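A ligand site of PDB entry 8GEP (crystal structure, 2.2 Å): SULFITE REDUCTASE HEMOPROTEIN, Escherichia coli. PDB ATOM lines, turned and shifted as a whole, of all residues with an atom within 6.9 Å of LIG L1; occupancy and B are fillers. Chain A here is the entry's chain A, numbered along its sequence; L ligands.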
ATOM      1  N   ALA A 360     -29.983 -12.439  15.318  1.00  0.00           N
ATOM      2  CA  ALA A 360     -29.203 -12.727  16.519  1.00  0.00           C
ATOM      3  C   ALA A 360     -29.854 -11.964  17.666  1.00  0.00           C
ATOM      4  O   ALA A 360     -30.519 -10.945  17.446  1.00  0.00           O
ATOM      5  CB  ALA A 360     -27.736 -12.272  16.361  1.00  0.00           C
ATOM      6  N   CYS A 361     -29.724 -12.508  18.867  1.00  0.00           N
ATOM      7  CA  CYS A 361     -30.290 -11.881  20.081  1.00  0.00           C
ATOM      8  C   CYS A 361     -29.412 -10.687  20.525  1.00  0.00           C
ATOM      9  O   CYS A 361     -28.352 -10.445  19.958  1.00  0.00           O
ATOM     10  CB  CYS A 361     -30.385 -12.892  21.209  1.00  0.00           C
ATOM     11  SG  CYS A 361     -28.790 -13.443  21.931  1.00  0.00           S
ATOM     12  N   VAL A 362     -29.859  -9.936  21.527  1.00  0.00           N
ATOM     13  CA  VAL A 362     -29.054  -8.805  22.001  1.00  0.00           C
ATOM     14  C   VAL A 362     -27.696  -9.273  22.518  1.00  0.00           C
ATOM     15  O   VAL A 362     -26.644  -8.875  21.975  1.00  0.00           O
ATOM     16  CB  VAL A 362     -29.793  -7.997  23.106  1.00  0.00           C
ATOM     17  CG1 VAL A 362     -28.825  -7.031  23.807  1.00  0.00           C
ATOM     18  CG2 VAL A 362     -30.976  -7.234  22.511  1.00  0.00           C
ATOM     19  N   SER A 363     -27.703 -10.118  23.552  1.00  0.00           N
ATOM     20  CA  SER A 363     -26.464 -10.637  24.131  1.00  0.00           C
ATOM     21  C   SER A 363     -25.595  -9.506  24.722  1.00  0.00           C
ATOM     22  O   SER A 363     -26.124  -8.552  25.298  1.00  0.00           O
ATOM     23  CB  SER A 363     -25.705 -11.456  23.083  1.00  0.00           C
ATOM     24  OG  SER A 363     -24.549 -12.052  23.644  1.00  0.00           O
ATOM     25  N   PHE A 364     -24.276  -9.637  24.653  1.00  0.00           N
ATOM     26  CA  PHE A 364     -23.345  -8.625  25.135  1.00  0.00           C
ATOM     27  C   PHE A 364     -23.594  -7.359  24.308  1.00  0.00           C
ATOM     28  O   PHE A 364     -23.830  -7.449  23.095  1.00  0.00           O
ATOM     29  CB  PHE A 364     -21.896  -9.072  24.921  1.00  0.00           C
ATOM     30  CG  PHE A 364     -21.514 -10.259  25.735  1.00  0.00           C
ATOM     31  CD1 PHE A 364     -21.310 -10.129  27.113  1.00  0.00           C
ATOM     32  CD2 PHE A 364     -21.344 -11.503  25.148  1.00  0.00           C
ATOM     33  CE1 PHE A 364     -20.919 -11.248  27.880  1.00  0.00           C
ATOM     34  CE2 PHE A 364     -20.963 -12.617  25.898  1.00  0.00           C
ATOM     35  CZ  PHE A 364     -20.753 -12.488  27.260  1.00  0.00           C
ATOM     36  N   THR A 366     -25.250  -5.726  27.001  1.00  0.00           N
ATOM     37  CA  THR A 366     -26.296  -5.522  28.012  1.00  0.00           C
ATOM     38  C   THR A 366     -26.866  -6.727  28.754  1.00  0.00           C
ATOM     39  O   THR A 366     -27.280  -6.599  29.903  1.00  0.00           O
ATOM     40  CB  THR A 366     -27.449  -4.695  27.439  1.00  0.00           C
ATOM     41  OG1 THR A 366     -27.886  -5.271  26.206  1.00  0.00           O
ATOM     42  CG2 THR A 366     -27.000  -3.265  27.163  1.00  0.00           C
ATOM     43  N   CYS A 367     -26.936  -7.893  28.098  1.00  0.00           N
ATOM     44  CA  CYS A 367     -27.500  -9.067  28.725  1.00  0.00           C
ATOM     45  C   CYS A 367     -26.598  -9.739  29.742  1.00  0.00           C
ATOM     46  O   CYS A 367     -25.549 -10.278  29.414  1.00  0.00           O
ATOM     47  CB  CYS A 367     -27.925 -10.109  27.695  1.00  0.00           C
ATOM     48  SG  CYS A 367     -28.793 -11.501  28.465  1.00  0.00           S
ATOM     49  N   PRO A 368     -27.089  -9.840  30.973  1.00  0.00           N
ATOM     50  CA  PRO A 368     -26.294 -10.467  32.022  1.00  0.00           C
ATOM     51  C   PRO A 368     -26.235 -11.990  31.950  1.00  0.00           C
ATOM     52  O   PRO A 368     -25.574 -12.653  32.757  1.00  0.00           O
ATOM     53  CB  PRO A 368     -27.000  -9.980  33.285  1.00  0.00           C
ATOM     54  CG  PRO A 368     -28.454  -9.963  32.835  1.00  0.00           C
ATOM     55  CD  PRO A 368     -28.361  -9.310  31.487  1.00  0.00           C
ATOM     56  N   LEU A 369     -26.932 -12.554  30.970  1.00  0.00           N
ATOM     57  CA  LEU A 369     -26.957 -13.997  30.864  1.00  0.00           C
ATOM     58  C   LEU A 369     -26.137 -14.445  29.686  1.00  0.00           C
ATOM     59  O   LEU A 369     -25.934 -15.638  29.494  1.00  0.00           O
ATOM     60  CB  LEU A 369     -28.397 -14.499  30.712  1.00  0.00           C
ATOM     61  CG  LEU A 369     -29.395 -13.917  31.725  1.00  0.00           C
ATOM     62  CD1 LEU A 369     -30.737 -14.608  31.616  1.00  0.00           C
ATOM     63  CD2 LEU A 369     -28.836 -14.045  33.122  1.00  0.00           C
ATOM     64  N   ALA A 370     -25.648 -13.508  28.896  1.00  0.00           N
ATOM     65  CA  ALA A 370     -24.893 -13.868  27.710  1.00  0.00           C
ATOM     66  C   ALA A 370     -23.636 -14.704  27.946  1.00  0.00           C
ATOM     67  O   ALA A 370     -22.959 -14.545  28.972  1.00  0.00           O
ATOM     68  CB  ALA A 370     -24.582 -12.623  26.886  1.00  0.00           C
ATOM     69  N   MET A 371     -23.347 -15.598  27.004  1.00  0.00           N
ATOM     70  CA  MET A 371     -22.168 -16.463  27.075  1.00  0.00           C
ATOM     71  C   MET A 371     -21.210 -16.168  25.918  1.00  0.00           C
ATOM     72  O   MET A 371     -19.994 -16.351  26.034  1.00  0.00           O
ATOM     73  CB  MET A 371     -22.614 -17.904  26.957  1.00  0.00           C
ATOM     74  CG  MET A 371     -23.456 -18.373  28.101  1.00  0.00           C
ATOM     75  SD  MET A 371     -23.923 -20.088  27.884  1.00  0.00           S
ATOM     76  CE  MET A 371     -24.171 -20.538  29.557  1.00  0.00           C
ATOM     77  N   ALA A 372     -21.780 -15.721  24.799  1.00  0.00           N
ATOM     78  CA  ALA A 372     -21.018 -15.421  23.586  1.00  0.00           C
ATOM     79  C   ALA A 372     -21.774 -14.309  22.866  1.00  0.00           C
ATOM     80  O   ALA A 372     -22.993 -14.180  23.041  1.00  0.00           O
ATOM     81  CB  ALA A 372     -20.933 -16.661  22.725  1.00  0.00           C
ATOM     82  N   ALA A 374     -23.678 -12.039  20.070  1.00  0.00           N
ATOM     83  CA  ALA A 374     -24.766 -12.373  19.158  1.00  0.00           C
ATOM     84  C   ALA A 374     -24.974 -11.218  18.188  1.00  0.00           C
ATOM     85  O   ALA A 374     -24.550 -11.276  17.053  1.00  0.00           O
ATOM     86  CB  ALA A 374     -26.049 -12.706  19.926  1.00  0.00           C
ATOM     87  N   VAL A 403     -28.244 -16.596  15.445  1.00  0.00           N
ATOM     88  CA  VAL A 403     -27.240 -16.671  16.490  1.00  0.00           C
ATOM     89  C   VAL A 403     -27.827 -16.308  17.826  1.00  0.00           C
ATOM     90  O   VAL A 403     -28.234 -15.166  18.036  1.00  0.00           O
ATOM     91  CB  VAL A 403     -26.124 -15.687  16.228  1.00  0.00           C
ATOM     92  CG1 VAL A 403     -25.083 -15.816  17.332  1.00  0.00           C
ATOM     93  CG2 VAL A 403     -25.541 -15.929  14.868  1.00  0.00           C
ATOM     94  N   THR A 404     -27.870 -17.278  18.727  1.00  0.00           N
ATOM     95  CA  THR A 404     -28.387 -17.001  20.055  1.00  0.00           C
ATOM     96  C   THR A 404     -27.219 -16.973  21.049  1.00  0.00           C
ATOM     97  O   THR A 404     -26.354 -17.807  21.012  1.00  0.00           O
ATOM     98  CB  THR A 404     -29.580 -17.954  20.399  1.00  0.00           C
ATOM     99  OG1 THR A 404     -30.430 -17.323  21.356  1.00  0.00           O
ATOM    100  CG2 THR A 404     -29.109 -19.324  20.887  1.00  0.00           C
ATOM    101  N   GLY A 405     -27.161 -15.902  21.821  1.00  0.00           N
ATOM    102  CA  GLY A 405     -26.093 -15.670  22.790  1.00  0.00           C
ATOM    103  C   GLY A 405     -25.839 -16.728  23.842  1.00  0.00           C
ATOM    104  O   GLY A 405     -24.678 -17.039  24.164  1.00  0.00           O
ATOM    105  N   CYS A 406     -26.918 -17.232  24.422  1.00  0.00           N
ATOM    106  CA  CYS A 406     -26.834 -18.279  25.427  1.00  0.00           C
ATOM    107  C   CYS A 406     -28.005 -19.213  25.143  1.00  0.00           C
ATOM    108  O   CYS A 406     -28.874 -18.939  24.310  1.00  0.00           O
ATOM    109  CB  CYS A 406     -26.898 -17.694  26.834  1.00  0.00           C
ATOM    110  SG  CYS A 406     -28.572 -17.218  27.320  1.00  0.00           S
ATOM    111  N   PRO A 407     -28.066 -20.354  25.849  1.00  0.00           N
ATOM    112  CA  PRO A 407     -29.168 -21.298  25.615  1.00  0.00           C
ATOM    113  C   PRO A 407     -30.594 -20.890  25.939  1.00  0.00           C
ATOM    114  O   PRO A 407     -31.530 -21.645  25.677  1.00  0.00           O
ATOM    115  CB  PRO A 407     -28.694 -22.522  26.373  1.00  0.00           C
ATOM    116  CG  PRO A 407     -27.998 -21.915  27.536  1.00  0.00           C
ATOM    117  CD  PRO A 407     -27.178 -20.853  26.899  1.00  0.00           C
ATOM    118  N   ASN A 408     -30.806 -19.686  26.456  1.00  0.00           N
ATOM    119  CA  ASN A 408     -32.159 -19.238  26.744  1.00  0.00           C
ATOM    120  C   ASN A 408     -32.934 -19.178  25.427  1.00  0.00           C
ATOM    121  O   ASN A 408     -34.163 -19.334  25.421  1.00  0.00           O
ATOM    122  CB  ASN A 408     -32.188 -17.899  27.475  1.00  0.00           C
ATOM    123  CG  ASN A 408     -31.762 -18.024  28.957  1.00  0.00           C
ATOM    124  OD1 ASN A 408     -31.866 -19.075  29.558  1.00  0.00           O
ATOM    125  ND2 ASN A 408     -31.290 -16.933  29.521  1.00  0.00           N
ATOM    126  N   GLY A 409     -32.213 -18.951  24.330  1.00  0.00           N
ATOM    127  CA  GLY A 409     -32.843 -18.972  23.009  1.00  0.00           C
ATOM    128  C   GLY A 409     -33.596 -17.782  22.418  1.00  0.00           C
ATOM    129  O   GLY A 409     -34.308 -17.956  21.434  1.00  0.00           O
ATOM    130  N   CYS A 410     -33.341 -16.591  22.915  1.00  0.00           N
ATOM    131  CA  CYS A 410     -33.989 -15.347  22.443  1.00  0.00           C
ATOM    132  C   CYS A 410     -33.799 -15.080  20.938  1.00  0.00           C
ATOM    133  O   CYS A 410     -34.629 -14.449  20.314  1.00  0.00           O
ATOM    134  CB  CYS A 410     -33.442 -14.174  23.250  1.00  0.00           C
ATOM    135  SG  CYS A 410     -33.556 -14.473  25.025  1.00  0.00           S
ATOM    136  N   GLY A 411     -32.723 -15.643  20.368  1.00  0.00           N
ATOM    137  CA  GLY A 411     -32.408 -15.474  18.964  1.00  0.00           C
ATOM    138  C   GLY A 411     -33.154 -16.435  18.038  1.00  0.00           C
ATOM    139  O   GLY A 411     -32.995 -16.376  16.811  1.00  0.00           O
HETATM  140 FE1  LIG L   1     -29.239 -13.615  24.088  1.00  0.00          FE
HETATM  141 FE2  LIG L   1     -29.190 -12.790  26.693  1.00  0.00          FE
HETATM  142 FE3  LIG L   1     -29.157 -15.362  26.249  1.00  0.00          FE
HETATM  143 FE4  LIG L   1     -31.464 -14.028  25.625  1.00  0.00          FE
HETATM  144  S1  LIG L   1     -30.600 -14.290  27.679  1.00  0.00           S
HETATM  145  S2  LIG L   1     -30.286 -15.623  24.387  1.00  0.00           S
HETATM  146  S3  LIG L   1     -30.514 -11.997  24.968  1.00  0.00           S
HETATM  147  S4  LIG L   1     -27.542 -13.850  25.513  1.00  0.00           S
HETATM  148 FE1  LG2 L   2     -35.712 -13.218  25.888  1.00  0.00          FE
HETATM  149  C1  LG2 L   2     -34.303 -13.369  29.124  1.00  0.00           C
HETATM  150  C2  LG2 L   2     -33.609 -10.381  25.358  1.00  0.00           C
HETATM  151  C3  LG2 L   2     -37.065 -12.870  22.829  1.00  0.00           C
HETATM  152  C4  LG2 L   2     -36.165 -16.475  25.878  1.00  0.00           C
HETATM  153  N1  LG2 L   2     -34.505 -11.932  27.110  1.00  0.00           N
HETATM  154  C5  LG2 L   2     -34.079 -12.252  28.369  1.00  0.00           C
HETATM  155  C6  LG2 L   2     -33.188 -11.208  28.958  1.00  0.00           C
HETATM  156  C7  LG2 L   2     -34.227 -10.183  29.548  1.00  0.00           C
HETATM  157  C8  LG2 L   2     -32.104 -11.498  29.991  1.00  0.00           C
HETATM  158  C9  LG2 L   2     -32.444 -11.325  31.470  1.00  0.00           C
HETATM  159  O1  LG2 L   2     -33.411 -11.965  31.940  1.00  0.00           O
HETATM  160  O2  LG2 L   2     -31.732 -10.548  32.171  1.00  0.00           O
HETATM  161  C10 LG2 L   2     -32.635 -10.504  27.734  1.00  0.00           C
HETATM  162  C11 LG2 L   2     -32.003  -9.141  27.858  1.00  0.00           C
HETATM  163  C12 LG2 L   2     -30.973  -8.519  26.942  1.00  0.00           C
HETATM  164  C13 LG2 L   2     -30.947  -7.011  27.065  1.00  0.00           C
HETATM  165  O3  LG2 L   2     -30.180  -6.501  27.912  1.00  0.00           O
HETATM  166  O4  LG2 L   2     -31.706  -6.326  26.337  1.00  0.00           O
HETATM  167  C14 LG2 L   2     -33.634 -10.952  26.637  1.00  0.00           C
HETATM  168  N2  LG2 L   2     -35.395 -11.794  24.357  1.00  0.00           N
HETATM  169  C15 LG2 L   2     -34.541 -10.704  24.375  1.00  0.00           C
HETATM  170  C16 LG2 L   2     -34.816  -9.967  23.088  1.00  0.00           C
HETATM  171  C17 LG2 L   2     -34.645  -8.473  23.286  1.00  0.00           C
HETATM  172  C18 LG2 L   2     -34.037 -10.718  22.046  1.00  0.00           C
HETATM  173  C19 LG2 L   2     -33.734  -9.902  20.816  1.00  0.00           C
HETATM  174  O5  LG2 L   2     -32.538  -9.754  20.526  1.00  0.00           O
HETATM  175  O6  LG2 L   2     -34.665  -9.408  20.157  1.00  0.00           O
HETATM  176  C20 LG2 L   2     -36.327 -10.362  22.974  1.00  0.00           C
HETATM  177  C21 LG2 L   2     -37.208  -9.648  24.022  1.00  0.00           C
HETATM  178  C22 LG2 L   2     -38.532  -9.915  23.327  1.00  0.00           C
HETATM  179  C23 LG2 L   2     -39.645  -9.000  23.812  1.00  0.00           C
HETATM  180  O7  LG2 L   2     -39.850  -7.937  23.204  1.00  0.00           O
HETATM  181  O8  LG2 L   2     -40.323  -9.376  24.768  1.00  0.00           O
HETATM  182  C24 LG2 L   2     -36.335 -11.823  23.351  1.00  0.00           C
HETATM  183  N3  LG2 L   2     -36.690 -14.490  24.561  1.00  0.00           N
HETATM  184  C25 LG2 L   2     -37.125 -14.140  23.329  1.00  0.00           C
HETATM  185  C26 LG2 L   2     -37.467 -15.346  22.700  1.00  0.00           C
HETATM  186  C27 LG2 L   2     -37.932 -15.466  21.271  1.00  0.00           C
HETATM  187  C28 LG2 L   2     -39.384 -14.990  21.082  1.00  0.00           C
HETATM  188  O9  LG2 L   2     -40.128 -14.883  22.069  1.00  0.00           O
HETATM  189  O10 LG2 L   2     -39.769 -14.730  19.940  1.00  0.00           O
HETATM  190  C29 LG2 L   2     -37.236 -16.434  23.503  1.00  0.00           C
HETATM  191  C30 LG2 L   2     -37.624 -17.823  23.010  1.00  0.00           C
HETATM  192  C31 LG2 L   2     -38.897 -18.673  23.216  1.00  0.00           C
HETATM  193  C32 LG2 L   2     -39.071 -19.110  24.663  1.00  0.00           C
HETATM  194  O11 LG2 L   2     -39.254 -18.212  25.527  1.00  0.00           O
HETATM  195  O12 LG2 L   2     -39.000 -20.335  24.946  1.00  0.00           O
HETATM  196  C33 LG2 L   2     -36.683 -15.876  24.706  1.00  0.00           C
HETATM  197  N4  LG2 L   2     -35.336 -14.668  27.362  1.00  0.00           N
HETATM  198  C34 LG2 L   2     -35.740 -15.957  27.138  1.00  0.00           C
HETATM  199  C35 LG2 L   2     -35.661 -16.625  28.410  1.00  0.00           C
HETATM  200  C36 LG2 L   2     -35.738 -18.184  28.621  1.00  0.00           C
HETATM  201  C37 LG2 L   2     -37.204 -18.432  28.873  1.00  0.00           C
HETATM  202  C38 LG2 L   2     -37.506 -19.755  29.535  1.00  0.00           C
HETATM  203  O13 LG2 L   2     -38.630 -20.248  29.380  1.00  0.00           O
HETATM  204  O14 LG2 L   2     -36.636 -20.292  30.221  1.00  0.00           O
HETATM  205  C39 LG2 L   2     -34.981 -15.766  29.289  1.00  0.00           C
HETATM  206  C40 LG2 L   2     -34.339 -16.123  30.655  1.00  0.00           C
HETATM  207  C41 LG2 L   2     -35.422 -16.295  31.694  1.00  0.00           C
HETATM  208  O15 LG2 L   2     -36.508 -15.708  31.511  1.00  0.00           O
HETATM  209  O16 LG2 L   2     -35.192 -17.016  32.697  1.00  0.00           O
HETATM  210  C42 LG2 L   2     -34.762 -14.557  28.610  1.00  0.00           C
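S2 of LIG L1 lies close to N of Cys 410, at 3.5 Å. SG of Cys 410 is bound to FE1 of LG2 L2. SG of Cys 406 binds FE3 of LIG L1 (2.2 Å). The backbone NH (N) of Ser 363 lies close to a sulfur (S3) of LIG L1 (3.7 Å). The side-chain sulfur (SG) of Cys 361 is bound to an iron atom (FE1) of LIG L1, 2.2 Å away. A sulfur (S4) of LIG L1 sits close to the backbone NH (N) of Cys 406 (3.6 Å). O3 of LG2 L2 sits at hydrogen-bond distance from OG1 of Thr 366 (3.1 Å). ND2 of Asn 408 sits close to S1 of LIG L1 (3.3 Å). The backbone NH (N) of Val 362 lies within hydrogen-bond range of an oxygen (O5) of LG2 L2, 2.9 Å away. An iron atom (FE4) of LIG L1 is bound by the side-chain sulfur (SG) of Cys 410. The side-chain hydroxyl (OG1) of Thr 404 lies close to a sulfur (S2) of LIG L1. SG of Cys 367 binds FE2 of LIG L1 (2.2 Å).
O of Val 403 lies within hydrogen-bond range of N of Cys 361. The side-chain sulfur (SG) of Cys 361 sits close to the backbone NH (N) of Gly 405, at 3.0 Å. The side-chain hydroxyl of Ser 363 sits at hydrogen-bond distance from the backbone carbonyl oxygen of Ala 372. The side-chain sulfur (SG) of Cys 406 lies close to the backbone NH (N) of Asn 408 (3.4 Å). N of Ala 370 lies close to SG of Cys 367 (3.8 Å). The backbone carbonyl oxygen of Gly 405 lies within hydrogen-bond range of the backbone NH of Met 371 (3.5 Å). O of Gly 405 sits at hydrogen-bond distance from N of Ala 372 (3.2 Å). O of Leu 369 sits close to SG of Cys 406 (3.8 Å).
Residues that only touch LIG L1: Leu 369, Ala 370, Gly 405 and Gly 409. Hydrophobic or aromatic side chains that line LIG L1: Leu 369 and Ala 370. 11 residues have an atom within 4 Å of LIG L1: Cys 361, Ser 363, Cys 367, Leu 369, Ala 370, Thr 404, Gly 405, Cys 406, Asn 408, Gly 409 and Cys 410. Along chain A the residues within 4 Å of LIG L1 span positions 361 to 410. The nearest printed residue that does not touch LIG L1 is Val 362 (4.1 Å).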
